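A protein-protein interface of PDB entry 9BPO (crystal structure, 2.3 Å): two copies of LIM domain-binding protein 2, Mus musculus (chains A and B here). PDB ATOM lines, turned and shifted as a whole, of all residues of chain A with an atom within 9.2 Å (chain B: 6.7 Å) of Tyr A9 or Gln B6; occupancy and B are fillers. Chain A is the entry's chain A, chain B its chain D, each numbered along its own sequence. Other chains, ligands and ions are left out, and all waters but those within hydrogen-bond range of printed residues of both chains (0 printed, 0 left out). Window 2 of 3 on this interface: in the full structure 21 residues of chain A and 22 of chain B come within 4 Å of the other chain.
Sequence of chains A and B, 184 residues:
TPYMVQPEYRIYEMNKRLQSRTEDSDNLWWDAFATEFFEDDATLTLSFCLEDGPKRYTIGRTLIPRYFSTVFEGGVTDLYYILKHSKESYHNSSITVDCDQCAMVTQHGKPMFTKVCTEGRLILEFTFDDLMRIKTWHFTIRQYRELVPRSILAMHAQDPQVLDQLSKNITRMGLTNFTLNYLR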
ATOM      1  N   MET A   4       7.266 -29.834  24.435  1.00  0.00           N
ATOM      2  CA  MET A   4       6.900 -29.368  23.104  1.00  0.00           C
ATOM      3  C   MET A   4       5.592 -28.612  23.224  1.00  0.00           C
ATOM      4  O   MET A   4       4.623 -29.151  23.762  1.00  0.00           O
ATOM      5  CB  MET A   4       6.766 -30.532  22.139  1.00  0.00           C
ATOM      6  CG  MET A   4       8.026 -30.787  21.370  1.00  0.00           C
ATOM      7  SD  MET A   4       7.668 -31.701  19.886  1.00  0.00           S
ATOM      8  CE  MET A   4       8.912 -31.062  18.769  1.00  0.00           C
ATOM      9  N   VAL A   5       5.581 -27.364  22.746  1.00  0.00           N
ATOM     10  CA  VAL A   5       4.351 -26.584  22.702  1.00  0.00           C
ATOM     11  C   VAL A   5       3.387 -27.237  21.728  1.00  0.00           C
ATOM     12  O   VAL A   5       3.757 -27.589  20.605  1.00  0.00           O
ATOM     13  CB  VAL A   5       4.641 -25.126  22.304  1.00  0.00           C
ATOM     14  CG1 VAL A   5       5.094 -24.326  23.503  1.00  0.00           C
ATOM     15  CG2 VAL A   5       5.689 -25.051  21.198  1.00  0.00           C
ATOM     16  N   GLN A   6       2.148 -27.428  22.154  1.00  0.00           N
ATOM     17  CA  GLN A   6       1.161 -27.823  21.163  1.00  0.00           C
ATOM     18  C   GLN A   6       0.724 -26.607  20.347  1.00  0.00           C
ATOM     19  O   GLN A   6       0.862 -25.454  20.795  1.00  0.00           O
ATOM     20  CB  GLN A   6      -0.032 -28.495  21.834  1.00  0.00           C
ATOM     21  CG  GLN A   6      -0.574 -27.880  23.075  1.00  0.00           C
ATOM     22  CD  GLN A   6      -1.349 -28.921  23.836  1.00  0.00           C
ATOM     23  OE1 GLN A   6      -1.359 -28.947  25.064  1.00  0.00           O
ATOM     24  NE2 GLN A   6      -2.009 -29.814  23.090  1.00  0.00           N
ATOM     25  N   PRO A   7       0.196 -26.831  19.139  1.00  0.00           N
ATOM     26  CA  PRO A   7       0.092 -25.708  18.203  1.00  0.00           C
ATOM     27  C   PRO A   7      -0.881 -24.623  18.636  1.00  0.00           C
ATOM     28  O   PRO A   7      -0.598 -23.437  18.397  1.00  0.00           O
ATOM     29  CB  PRO A   7      -0.335 -26.370  16.890  1.00  0.00           C
ATOM     30  CG  PRO A   7      -0.698 -27.802  17.244  1.00  0.00           C
ATOM     31  CD  PRO A   7      -0.673 -27.942  18.733  1.00  0.00           C
ATOM     32  N   GLU A   8      -1.975 -24.960  19.327  1.00  0.00           N
ATOM     33  CA  GLU A   8      -2.897 -23.894  19.710  1.00  0.00           C
ATOM     34  C   GLU A   8      -2.245 -22.894  20.672  1.00  0.00           C
ATOM     35  O   GLU A   8      -2.532 -21.695  20.599  1.00  0.00           O
ATOM     36  CB  GLU A   8      -4.187 -24.475  20.295  1.00  0.00           C
ATOM     37  N   TYR A   9      -1.345 -23.351  21.548  1.00  0.00           N
ATOM     38  CA  TYR A   9      -0.602 -22.419  22.391  1.00  0.00           C
ATOM     39  C   TYR A   9       0.272 -21.476  21.564  1.00  0.00           C
ATOM     40  O   TYR A   9       0.498 -20.327  21.964  1.00  0.00           O
ATOM     41  CB  TYR A   9       0.263 -23.183  23.397  1.00  0.00           C
ATOM     42  CG  TYR A   9       0.957 -22.301  24.429  1.00  0.00           C
ATOM     43  CD1 TYR A   9       0.326 -21.958  25.615  1.00  0.00           C
ATOM     44  CD2 TYR A   9       2.248 -21.827  24.220  1.00  0.00           C
ATOM     45  CE1 TYR A   9       0.942 -21.157  26.549  1.00  0.00           C
ATOM     46  CE2 TYR A   9       2.876 -21.030  25.159  1.00  0.00           C
ATOM     47  CZ  TYR A   9       2.211 -20.697  26.317  1.00  0.00           C
ATOM     48  OH  TYR A   9       2.819 -19.908  27.258  1.00  0.00           O
ATOM     49  N   ARG A  10       0.781 -21.936  20.415  1.00  0.00           N
ATOM     50  CA  ARG A  10       1.577 -21.045  19.575  1.00  0.00           C
ATOM     51  C   ARG A  10       0.748 -19.854  19.119  1.00  0.00           C
ATOM     52  O   ARG A  10       1.260 -18.734  19.036  1.00  0.00           O
ATOM     53  CB  ARG A  10       2.150 -21.799  18.370  1.00  0.00           C
ATOM     54  CG  ARG A  10       3.222 -22.823  18.728  1.00  0.00           C
ATOM     55  CD  ARG A  10       4.470 -22.148  19.317  1.00  0.00           C
ATOM     56  NE  ARG A  10       5.313 -21.537  18.294  1.00  0.00           N
ATOM     57  CZ  ARG A  10       5.933 -20.368  18.412  1.00  0.00           C
ATOM     58  NH1 ARG A  10       5.832 -19.629  19.514  1.00  0.00           N
ATOM     59  NH2 ARG A  10       6.682 -19.927  17.404  1.00  0.00           N
ATOM     60  N   ILE A  11      -0.543 -20.079  18.839  1.00  0.00           N
ATOM     61  CA  ILE A  11      -1.409 -19.024  18.320  1.00  0.00           C
ATOM     62  C   ILE A  11      -1.756 -18.026  19.415  1.00  0.00           C
ATOM     63  O   ILE A  11      -1.810 -16.814  19.176  1.00  0.00           O
ATOM     64  CB  ILE A  11      -2.676 -19.648  17.704  1.00  0.00           C
ATOM     65  CG1 ILE A  11      -2.303 -20.546  16.540  1.00  0.00           C
ATOM     66  CG2 ILE A  11      -3.632 -18.554  17.169  1.00  0.00           C
ATOM     67  CD1 ILE A  11      -1.824 -19.740  15.377  1.00  0.00           C
ATOM     68  N   TYR A  12      -2.040 -18.519  20.620  1.00  0.00           N
ATOM     69  CA  TYR A  12      -2.187 -17.628  21.761  1.00  0.00           C
ATOM     70  C   TYR A  12      -0.934 -16.791  21.942  1.00  0.00           C
ATOM     71  O   TYR A  12      -1.014 -15.609  22.293  1.00  0.00           O
ATOM     72  CB  TYR A  12      -2.483 -18.432  23.032  1.00  0.00           C
ATOM     73  CG  TYR A  12      -2.004 -17.791  24.328  1.00  0.00           C
ATOM     74  CD1 TYR A  12      -0.722 -18.039  24.824  1.00  0.00           C
ATOM     75  CD2 TYR A  12      -2.834 -16.962  25.069  1.00  0.00           C
ATOM     76  CE1 TYR A  12      -0.277 -17.458  26.015  1.00  0.00           C
ATOM     77  CE2 TYR A  12      -2.395 -16.379  26.278  1.00  0.00           C
ATOM     78  CZ  TYR A  12      -1.123 -16.631  26.740  1.00  0.00           C
ATOM     79  OH  TYR A  12      -0.670 -16.069  27.918  1.00  0.00           O
ATOM     80  N   GLU A  13       0.234 -17.395  21.723  1.00  0.00           N
ATOM     81  CA  GLU A  13       1.471 -16.633  21.797  1.00  0.00           C
ATOM     82  C   GLU A  13       1.501 -15.543  20.740  1.00  0.00           C
ATOM     83  O   GLU A  13       2.002 -14.439  20.983  1.00  0.00           O
ATOM     84  CB  GLU A  13       2.669 -17.563  21.626  1.00  0.00           C
ATOM     85  CG  GLU A  13       2.913 -18.484  22.802  1.00  0.00           C
ATOM     86  CD  GLU A  13       4.322 -19.058  22.778  1.00  0.00           C
ATOM     87  OE1 GLU A  13       4.641 -19.749  21.782  1.00  0.00           O
ATOM     88  OE2 GLU A  13       5.104 -18.795  23.724  1.00  0.00           O
ATOM     89  N   MET A  14       0.995 -15.848  19.550  1.00  0.00           N
ATOM     90  CA  MET A  14       1.030 -14.871  18.476  1.00  0.00           C
ATOM     91  C   MET A  14       0.055 -13.729  18.760  1.00  0.00           C
ATOM     92  O   MET A  14       0.400 -12.561  18.570  1.00  0.00           O
ATOM     93  CB  MET A  14       0.755 -15.579  17.145  1.00  0.00           C
ATOM     94  CG  MET A  14       0.106 -14.749  16.046  1.00  0.00           C
ATOM     95  SD  MET A  14       0.697 -15.229  14.393  1.00  0.00           S
ATOM     96  CE  MET A  14       0.173 -16.936  14.347  1.00  0.00           C
ATOM     97  N   ASN A  15      -1.134 -14.047  19.284  1.00  0.00           N
ATOM     98  CA  ASN A  15      -2.060 -13.009  19.734  1.00  0.00           C
ATOM     99  C   ASN A  15      -1.436 -12.150  20.837  1.00  0.00           C
ATOM    100  O   ASN A  15      -1.520 -10.916  20.803  1.00  0.00           O
ATOM    101  CB  ASN A  15      -3.362 -13.647  20.225  1.00  0.00           C
ATOM    102  CG  ASN A  15      -4.277 -14.080  19.097  1.00  0.00           C
ATOM    103  OD1 ASN A  15      -4.186 -13.586  17.972  1.00  0.00           O
ATOM    104  ND2 ASN A  15      -5.167 -15.019  19.391  1.00  0.00           N
ATOM    105  N   LYS A  16      -0.768 -12.786  21.802  1.00  0.00           N
ATOM    106  CA  LYS A  16      -0.133 -12.039  22.883  1.00  0.00           C
ATOM    107  C   LYS A  16       0.959 -11.125  22.348  1.00  0.00           C
ATOM    108  O   LYS A  16       1.120  -9.991  22.810  1.00  0.00           O
ATOM    109  CB  LYS A  16       0.433 -13.005  23.926  1.00  0.00           C
ATOM    110  CG  LYS A  16       0.452 -12.420  25.314  1.00  0.00           C
ATOM    111  N   ARG A  17       1.712 -11.593  21.363  1.00  0.00           N
ATOM    112  CA  ARG A  17       2.769 -10.764  20.799  1.00  0.00           C
ATOM    113  C   ARG A  17       2.183  -9.596  20.006  1.00  0.00           C
ATOM    114  O   ARG A  17       2.699  -8.478  20.065  1.00  0.00           O
ATOM    115  CB  ARG A  17       3.692 -11.636  19.940  1.00  0.00           C
ATOM    116  CG  ARG A  17       4.944 -10.955  19.452  1.00  0.00           C
ATOM    117  CD  ARG A  17       6.066 -11.090  20.461  1.00  0.00           C
ATOM    118  NE  ARG A  17       6.889  -9.886  20.475  1.00  0.00           N
ATOM    119  CZ  ARG A  17       7.415  -9.330  21.562  1.00  0.00           C
ATOM    120  NH1 ARG A  17       7.228  -9.848  22.768  1.00  0.00           N
ATOM    121  NH2 ARG A  17       8.138  -8.217  21.437  1.00  0.00           N
ATOM    122  N   GLU A  36       9.935 -14.951  14.859  1.00  0.00           N
ATOM    123  CA  GLU A  36       9.478 -15.718  16.010  1.00  0.00           C
ATOM    124  C   GLU A  36       8.508 -16.818  15.586  1.00  0.00           C
ATOM    125  O   GLU A  36       8.568 -17.942  16.101  1.00  0.00           O
ATOM    126  CB  GLU A  36       8.833 -14.780  17.038  1.00  0.00           C
ATOM    127  CG  GLU A  36       8.251 -15.478  18.278  1.00  0.00           C
ATOM    128  CD  GLU A  36       8.007 -14.518  19.488  1.00  0.00           C
ATOM    129  OE1 GLU A  36       8.126 -13.262  19.346  1.00  0.00           O
ATOM    130  OE2 GLU A  36       7.694 -15.031  20.601  1.00  0.00           O
ATOM    131  N   PHE A  37       7.638 -16.533  14.609  1.00  0.00           N
ATOM    132  CA  PHE A  37       6.495 -17.398  14.336  1.00  0.00           C
ATOM    133  C   PHE A  37       6.508 -18.097  12.979  1.00  0.00           C
ATOM    134  O   PHE A  37       5.787 -19.085  12.815  1.00  0.00           O
ATOM    135  CB  PHE A  37       5.192 -16.592  14.469  1.00  0.00           C
ATOM    136  CG  PHE A  37       4.933 -16.100  15.870  1.00  0.00           C
ATOM    137  CD1 PHE A  37       4.430 -16.956  16.840  1.00  0.00           C
ATOM    138  CD2 PHE A  37       5.203 -14.796  16.215  1.00  0.00           C
ATOM    139  CE1 PHE A  37       4.207 -16.519  18.126  1.00  0.00           C
ATOM    140  CE2 PHE A  37       4.974 -14.344  17.498  1.00  0.00           C
ATOM    141  CZ  PHE A  37       4.484 -15.209  18.457  1.00  0.00           C
ATOM    142  N   LEU A  83      -9.840 -18.952  16.694  1.00  0.00           N
ATOM    143  CA  LEU A  83      -9.985 -20.208  15.963  1.00  0.00           C
ATOM    144  C   LEU A  83     -11.033 -21.062  16.661  1.00  0.00           C
ATOM    145  O   LEU A  83     -10.864 -21.428  17.829  1.00  0.00           O
ATOM    146  CB  LEU A  83      -8.661 -20.968  15.887  1.00  0.00           C
ATOM    147  CG  LEU A  83      -7.412 -20.269  15.365  1.00  0.00           C
ATOM    148  CD1 LEU A  83      -6.332 -21.289  15.146  1.00  0.00           C
ATOM    149  CD2 LEU A  83      -7.727 -19.607  14.084  1.00  0.00           C
ATOM    150  N   GLU A  88      -6.387 -30.675  14.543  1.00  0.00           N
ATOM    151  CA  GLU A  88      -4.951 -30.880  14.398  1.00  0.00           C
ATOM    152  C   GLU A  88      -4.703 -32.248  13.787  1.00  0.00           C
ATOM    153  O   GLU A  88      -5.363 -33.223  14.147  1.00  0.00           O
ATOM    154  CB  GLU A  88      -4.221 -30.810  15.743  1.00  0.00           C
ATOM    155  CG  GLU A  88      -4.461 -29.575  16.585  1.00  0.00           C
ATOM    156  CD  GLU A  88      -4.099 -29.836  18.041  1.00  0.00           C
ATOM    157  OE1 GLU A  88      -3.615 -30.967  18.337  1.00  0.00           O
ATOM    158  OE2 GLU A  88      -4.293 -28.924  18.883  1.00  0.00           O
ATOM    159  N   VAL A  97      -2.941 -27.375  11.489  1.00  0.00           N
ATOM    160  CA  VAL A  97      -4.076 -26.861  12.239  1.00  0.00           C
ATOM    161  C   VAL A  97      -5.078 -26.347  11.219  1.00  0.00           C
ATOM    162  O   VAL A  97      -4.820 -25.371  10.499  1.00  0.00           O
ATOM    163  CB  VAL A  97      -3.666 -25.767  13.231  1.00  0.00           C
ATOM    164  CG1 VAL A  97      -4.909 -25.112  13.829  1.00  0.00           C
ATOM    165  CG2 VAL A  97      -2.813 -26.370  14.332  1.00  0.00           C
ATOM    166  N   PHE A 126       2.507 -26.182  10.785  1.00  0.00           N
ATOM    167  CA  PHE A 126       3.652 -26.013  11.672  1.00  0.00           C
ATOM    168  C   PHE A 126       4.680 -27.112  11.449  1.00  0.00           C
ATOM    169  O   PHE A 126       4.342 -28.231  11.067  1.00  0.00           O
ATOM    170  CB  PHE A 126       3.237 -26.065  13.136  1.00  0.00           C
ATOM    171  CG  PHE A 126       2.315 -24.977  13.532  1.00  0.00           C
ATOM    172  CD1 PHE A 126       0.964 -25.041  13.196  1.00  0.00           C
ATOM    173  CD2 PHE A 126       2.785 -23.881  14.239  1.00  0.00           C
ATOM    174  CE1 PHE A 126       0.118 -24.053  13.566  1.00  0.00           C
ATOM    175  CE2 PHE A 126       1.930 -22.880  14.601  1.00  0.00           C
ATOM    176  CZ  PHE A 126       0.603 -22.967  14.271  1.00  0.00           C
ATOM    177  N   LEU A 131      11.089 -25.210  17.908  1.00  0.00           N
ATOM    178  CA  LEU A 131      10.664 -23.824  17.752  1.00  0.00           C
ATOM    179  C   LEU A 131       9.178 -23.726  17.419  1.00  0.00           C
ATOM    180  O   LEU A 131       8.483 -22.851  17.945  1.00  0.00           O
ATOM    181  CB  LEU A 131      11.492 -23.140  16.667  1.00  0.00           C
ATOM    182  CG  LEU A 131      12.915 -22.746  17.050  1.00  0.00           C
ATOM    183  CD1 LEU A 131      13.387 -21.573  16.199  1.00  0.00           C
ATOM    184  CD2 LEU A 131      13.001 -22.425  18.526  1.00  0.00           C
ATOM    185  N   MET A 132       8.689 -24.615  16.554  1.00  0.00           N
ATOM    186  CA  MET A 132       7.275 -24.702  16.219  1.00  0.00           C
ATOM    187  C   MET A 132       6.783 -23.486  15.465  1.00  0.00           C
ATOM    188  O   MET A 132       5.911 -22.760  15.946  1.00  0.00           O
ATOM    189  CB  MET A 132       6.444 -24.892  17.474  1.00  0.00           C
ATOM    190  CG  MET A 132       6.078 -26.294  17.652  1.00  0.00           C
ATOM    191  SD  MET A 132       4.526 -26.583  16.814  1.00  0.00           S
ATOM    192  CE  MET A 132       4.168 -28.161  17.587  1.00  0.00           C
ATOM    193  N   MET B   4       8.503 -22.593  34.185  1.00  0.00           N
ATOM    194  CA  MET B   4       7.775 -21.669  33.320  1.00  0.00           C
ATOM    195  C   MET B   4       6.302 -22.044  33.203  1.00  0.00           C
ATOM    196  O   MET B   4       5.901 -22.742  32.277  1.00  0.00           O
ATOM    197  CB  MET B   4       8.419 -21.615  31.929  1.00  0.00           C
ATOM    198  CG  MET B   4       9.266 -22.831  31.573  1.00  0.00           C
ATOM    199  SD  MET B   4       9.831 -22.809  29.860  1.00  0.00           S
ATOM    200  CE  MET B   4      11.164 -21.615  29.947  1.00  0.00           C
ATOM    201  N   VAL B   5       5.500 -21.566  34.147  1.00  0.00           N
ATOM    202  CA  VAL B   5       4.061 -21.825  34.173  1.00  0.00           C
ATOM    203  C   VAL B   5       3.320 -20.578  33.693  1.00  0.00           C
ATOM    204  O   VAL B   5       3.728 -19.447  33.999  1.00  0.00           O
ATOM    205  CB  VAL B   5       3.617 -22.258  35.586  1.00  0.00           C
ATOM    206  CG1 VAL B   5       3.591 -21.075  36.558  1.00  0.00           C
ATOM    207  CG2 VAL B   5       2.278 -22.961  35.536  1.00  0.00           C
ATOM    208  N   GLN B   6       2.242 -20.773  32.927  1.00  0.00           N
ATOM    209  CA  GLN B   6       1.575 -19.670  32.227  1.00  0.00           C
ATOM    210  C   GLN B   6       0.082 -19.587  32.551  1.00  0.00           C
ATOM    211  O   GLN B   6      -0.746 -20.255  31.906  1.00  0.00           O
ATOM    212  CB  GLN B   6       1.800 -19.778  30.720  1.00  0.00           C
ATOM    213  CG  GLN B   6       2.771 -18.732  30.177  1.00  0.00           C
ATOM    214  CD  GLN B   6       2.204 -17.300  30.191  1.00  0.00           C
ATOM    215  OE1 GLN B   6       1.153 -17.017  30.790  1.00  0.00           O
ATOM    216  NE2 GLN B   6       2.935 -16.382  29.562  1.00  0.00           N
ATOM    217  N   PRO B   7      -0.305 -18.742  33.499  1.00  0.00           N
ATOM    218  CA  PRO B   7      -1.671 -18.802  34.040  1.00  0.00           C
ATOM    219  C   PRO B   7      -2.726 -18.207  33.128  1.00  0.00           C
ATOM    220  O   PRO B   7      -3.890 -18.612  33.178  1.00  0.00           O
ATOM    221  CB  PRO B   7      -1.570 -18.004  35.348  1.00  0.00           C
ATOM    222  CG  PRO B   7      -0.162 -17.447  35.399  1.00  0.00           C
ATOM    223  CD  PRO B   7       0.477 -17.640  34.071  1.00  0.00           C
ATOM    224  N   GLU B   8      -2.334 -17.241  32.298  1.00  0.00           N
ATOM    225  CA  GLU B   8      -3.302 -16.579  31.434  1.00  0.00           C
ATOM    226  C   GLU B   8      -3.892 -17.553  30.422  1.00  0.00           C
ATOM    227  O   GLU B   8      -5.067 -17.429  30.051  1.00  0.00           O
ATOM    228  CB  GLU B   8      -2.635 -15.392  30.736  1.00  0.00           C
ATOM    229  CG  GLU B   8      -3.403 -14.810  29.551  1.00  0.00           C
ATOM    230  CD  GLU B   8      -2.747 -13.554  28.974  1.00  0.00           C
ATOM    231  OE1 GLU B   8      -3.016 -13.227  27.793  1.00  0.00           O
ATOM    232  OE2 GLU B   8      -1.960 -12.901  29.700  1.00  0.00           O
ATOM    233  N   TYR B   9      -3.101 -18.544  29.994  1.00  0.00           N
ATOM    234  CA  TYR B   9      -3.578 -19.546  29.047  1.00  0.00           C
ATOM    235  C   TYR B   9      -4.792 -20.309  29.569  1.00  0.00           C
ATOM    236  O   TYR B   9      -5.623 -20.760  28.772  1.00  0.00           O
ATOM    237  CB  TYR B   9      -2.445 -20.514  28.720  1.00  0.00           C
ATOM    238  CG  TYR B   9      -2.744 -21.569  27.666  1.00  0.00           C
ATOM    239  CD1 TYR B   9      -2.958 -21.230  26.328  1.00  0.00           C
ATOM    240  CD2 TYR B   9      -2.768 -22.921  28.006  1.00  0.00           C
ATOM    241  CE1 TYR B   9      -3.206 -22.217  25.362  1.00  0.00           C
ATOM    242  CE2 TYR B   9      -3.016 -23.902  27.057  1.00  0.00           C
ATOM    243  CZ  TYR B   9      -3.240 -23.551  25.736  1.00  0.00           C
ATOM    244  OH  TYR B   9      -3.478 -24.550  24.800  1.00  0.00           O
ATOM    245  N   ARG B  10      -4.904 -20.482  30.892  1.00  0.00           N
ATOM    246  CA  ARG B  10      -6.117 -21.056  31.475  1.00  0.00           C
ATOM    247  C   ARG B  10      -7.386 -20.401  30.930  1.00  0.00           C
ATOM    248  O   ARG B  10      -8.420 -21.064  30.803  1.00  0.00           O
ATOM    249  CB  ARG B  10      -6.086 -20.906  32.998  1.00  0.00           C
ATOM    250  CG  ARG B  10      -5.283 -21.959  33.735  1.00  0.00           C
ATOM    251  CD  ARG B  10      -5.650 -23.360  33.273  1.00  0.00           C
ATOM    252  NE  ARG B  10      -6.666 -23.970  34.121  1.00  0.00           N
ATOM    253  CZ  ARG B  10      -7.553 -24.854  33.691  1.00  0.00           C
ATOM    254  NH1 ARG B  10      -7.574 -25.250  32.430  1.00  0.00           N
ATOM    255  NH2 ARG B  10      -8.443 -25.351  34.544  1.00  0.00           N
ATOM    256  N   TYR B  12      -7.582 -18.849  27.884  1.00  0.00           N
ATOM    257  CA  TYR B  12      -7.665 -19.368  26.527  1.00  0.00           C
ATOM    258  C   TYR B  12      -8.357 -20.720  26.508  1.00  0.00           C
ATOM    259  O   TYR B  12      -9.203 -20.984  25.644  1.00  0.00           O
ATOM    260  CB  TYR B  12      -6.265 -19.461  25.930  1.00  0.00           C
ATOM    261  CG  TYR B  12      -6.182 -19.769  24.450  1.00  0.00           C
ATOM    262  CD1 TYR B  12      -5.965 -18.741  23.525  1.00  0.00           C
ATOM    263  CD2 TYR B  12      -6.222 -21.090  23.982  1.00  0.00           C
ATOM    264  CE1 TYR B  12      -5.858 -19.008  22.165  1.00  0.00           C
ATOM    265  CE2 TYR B  12      -6.112 -21.375  22.624  1.00  0.00           C
ATOM    266  CZ  TYR B  12      -5.923 -20.331  21.715  1.00  0.00           C
ATOM    267  OH  TYR B  12      -5.799 -20.609  20.359  1.00  0.00           O
ATOM    268  N   GLU B  88       1.102 -10.969  36.041  1.00  0.00           N
ATOM    269  CA  GLU B  88       0.989 -12.209  36.798  1.00  0.00           C
ATOM    270  C   GLU B  88       1.792 -12.100  38.088  1.00  0.00           C
ATOM    271  O   GLU B  88       2.900 -11.561  38.096  1.00  0.00           O
ATOM    272  CB  GLU B  88       1.460 -13.405  35.961  1.00  0.00           C
ATOM    273  N   TYR B  90       2.891 -14.327  41.769  1.00  0.00           N
ATOM    274  CA  TYR B  90       2.993 -15.616  42.435  1.00  0.00           C
ATOM    275  C   TYR B  90       3.113 -15.384  43.933  1.00  0.00           C
ATOM    276  O   TYR B  90       3.966 -14.609  44.380  1.00  0.00           O
ATOM    277  CB  TYR B  90       4.186 -16.418  41.895  1.00  0.00           C
ATOM    278  CG  TYR B  90       4.056 -16.707  40.414  1.00  0.00           C
ATOM    279  CD1 TYR B  90       3.637 -17.954  39.961  1.00  0.00           C
ATOM    280  CD2 TYR B  90       4.315 -15.717  39.463  1.00  0.00           C
ATOM    281  CE1 TYR B  90       3.482 -18.214  38.590  1.00  0.00           C
ATOM    282  CE2 TYR B  90       4.165 -15.963  38.100  1.00  0.00           C
ATOM    283  CZ  TYR B  90       3.748 -17.212  37.665  1.00  0.00           C
ATOM    284  OH  TYR B  90       3.609 -17.472  36.312  1.00  0.00           O
ATOM    285  N   MET B 132      -4.965 -25.737  38.578  1.00  0.00           N
ATOM    286  CA  MET B 132      -4.924 -24.289  38.356  1.00  0.00           C
ATOM    287  C   MET B 132      -6.321 -23.712  38.114  1.00  0.00           C
ATOM    288  O   MET B 132      -6.597 -23.074  37.098  1.00  0.00           O
ATOM    289  CB  MET B 132      -4.003 -23.939  37.189  1.00  0.00           C
ATOM    290  CG  MET B 132      -3.260 -22.631  37.395  1.00  0.00           C
ATOM    291  SD  MET B 132      -1.998 -22.448  36.132  1.00  0.00           S
ATOM    292  CE  MET B 132      -0.599 -21.958  37.106  1.00  0.00           C
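Tyr A9 touches Gln B6, but with the chains exchanged Gln A6 does not touch Tyr B9 (4.7 Å).
Tyr A9 touches its own counterpart, Tyr B9.
Tyr A12 touches Gln B6, but with the chains exchanged Gln A6 does not touch Tyr B12 (8.2 Å).
Tyr B12 touches its own counterpart, Tyr A12.
Positions printed for both chains: 4, 5, 6, 7, 8, 9, 10, 12, 88 and 132.
Of the 6 pairs that touch across the chains among the printed residues, 4 have their exchanged pair printed and touching as well.
Among the printed residues, merely in contact across the chains: Tyr A9 with Gln B6 (3.1 Å), Tyr A9 with Tyr B9 (3.4 Å), Tyr A12 with Gln B6 (3.5 Å), Tyr A12 with Glu B8 (3.4 Å) and Tyr A12 with Tyr B12 (3.5 Å).
The backbone carbonyl oxygen (O) of Glu A8 lies within hydrogen-bond range of the side-chain hydroxyl (OH) of Tyr B12 (3.5 Å).
Hydrophobic or aromatic side chains of chain A that line the printed part of chain B: Tyr A9 and Tyr A12.
Printed residues of chain B that touch a printed residue of chain A: Gln B6, Glu B8, Tyr B9 and Tyr B12.
Hydrophobic or aromatic side chains of chain B within 4 Å of the printed part of chain A: Tyr B9 and Tyr B12.
Among the printed residues, no Asp or Glu carboxylate lies within 4 Å of a Lys or Arg side-chain nitrogen of the other chain.
Tyr A9 touches two residues of chain B.
Of chain A, only Tyr A9 (3.1 Å) and Tyr A12 (3.5 Å) come within 4 Å of Gln B6.
No residue of chain A comes within 4 Å of Val B5.
No residue of chain A comes within 4 Å of Pro B7.
Of the printed residues of chain A, Tyr B12 touches Glu A8 (3.5 Å) and Tyr A12 (3.5 Å).
Of the printed residues of chain B, Tyr A12 touches Gln B6 (3.5 Å), Glu B8 (3.4 Å) and Tyr B12 (3.5 Å).
Of the printed residues of chain B, Glu A8 touches Tyr B12.
Of the printed residues of chain A, Tyr B9 touches Tyr A9.
Tyr B90 touches none of the printed residues of chain A.
The nearest residue of chain B that does not touch Tyr A9 is Tyr B12 (5.3 Å).
The nearest residue of chain A that does not touch Gln B6 is Lys A16 (6.3 Å).
The nearest printed residue of chain B that does not touch Glu A8 is Tyr B9 (4.6 Å).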
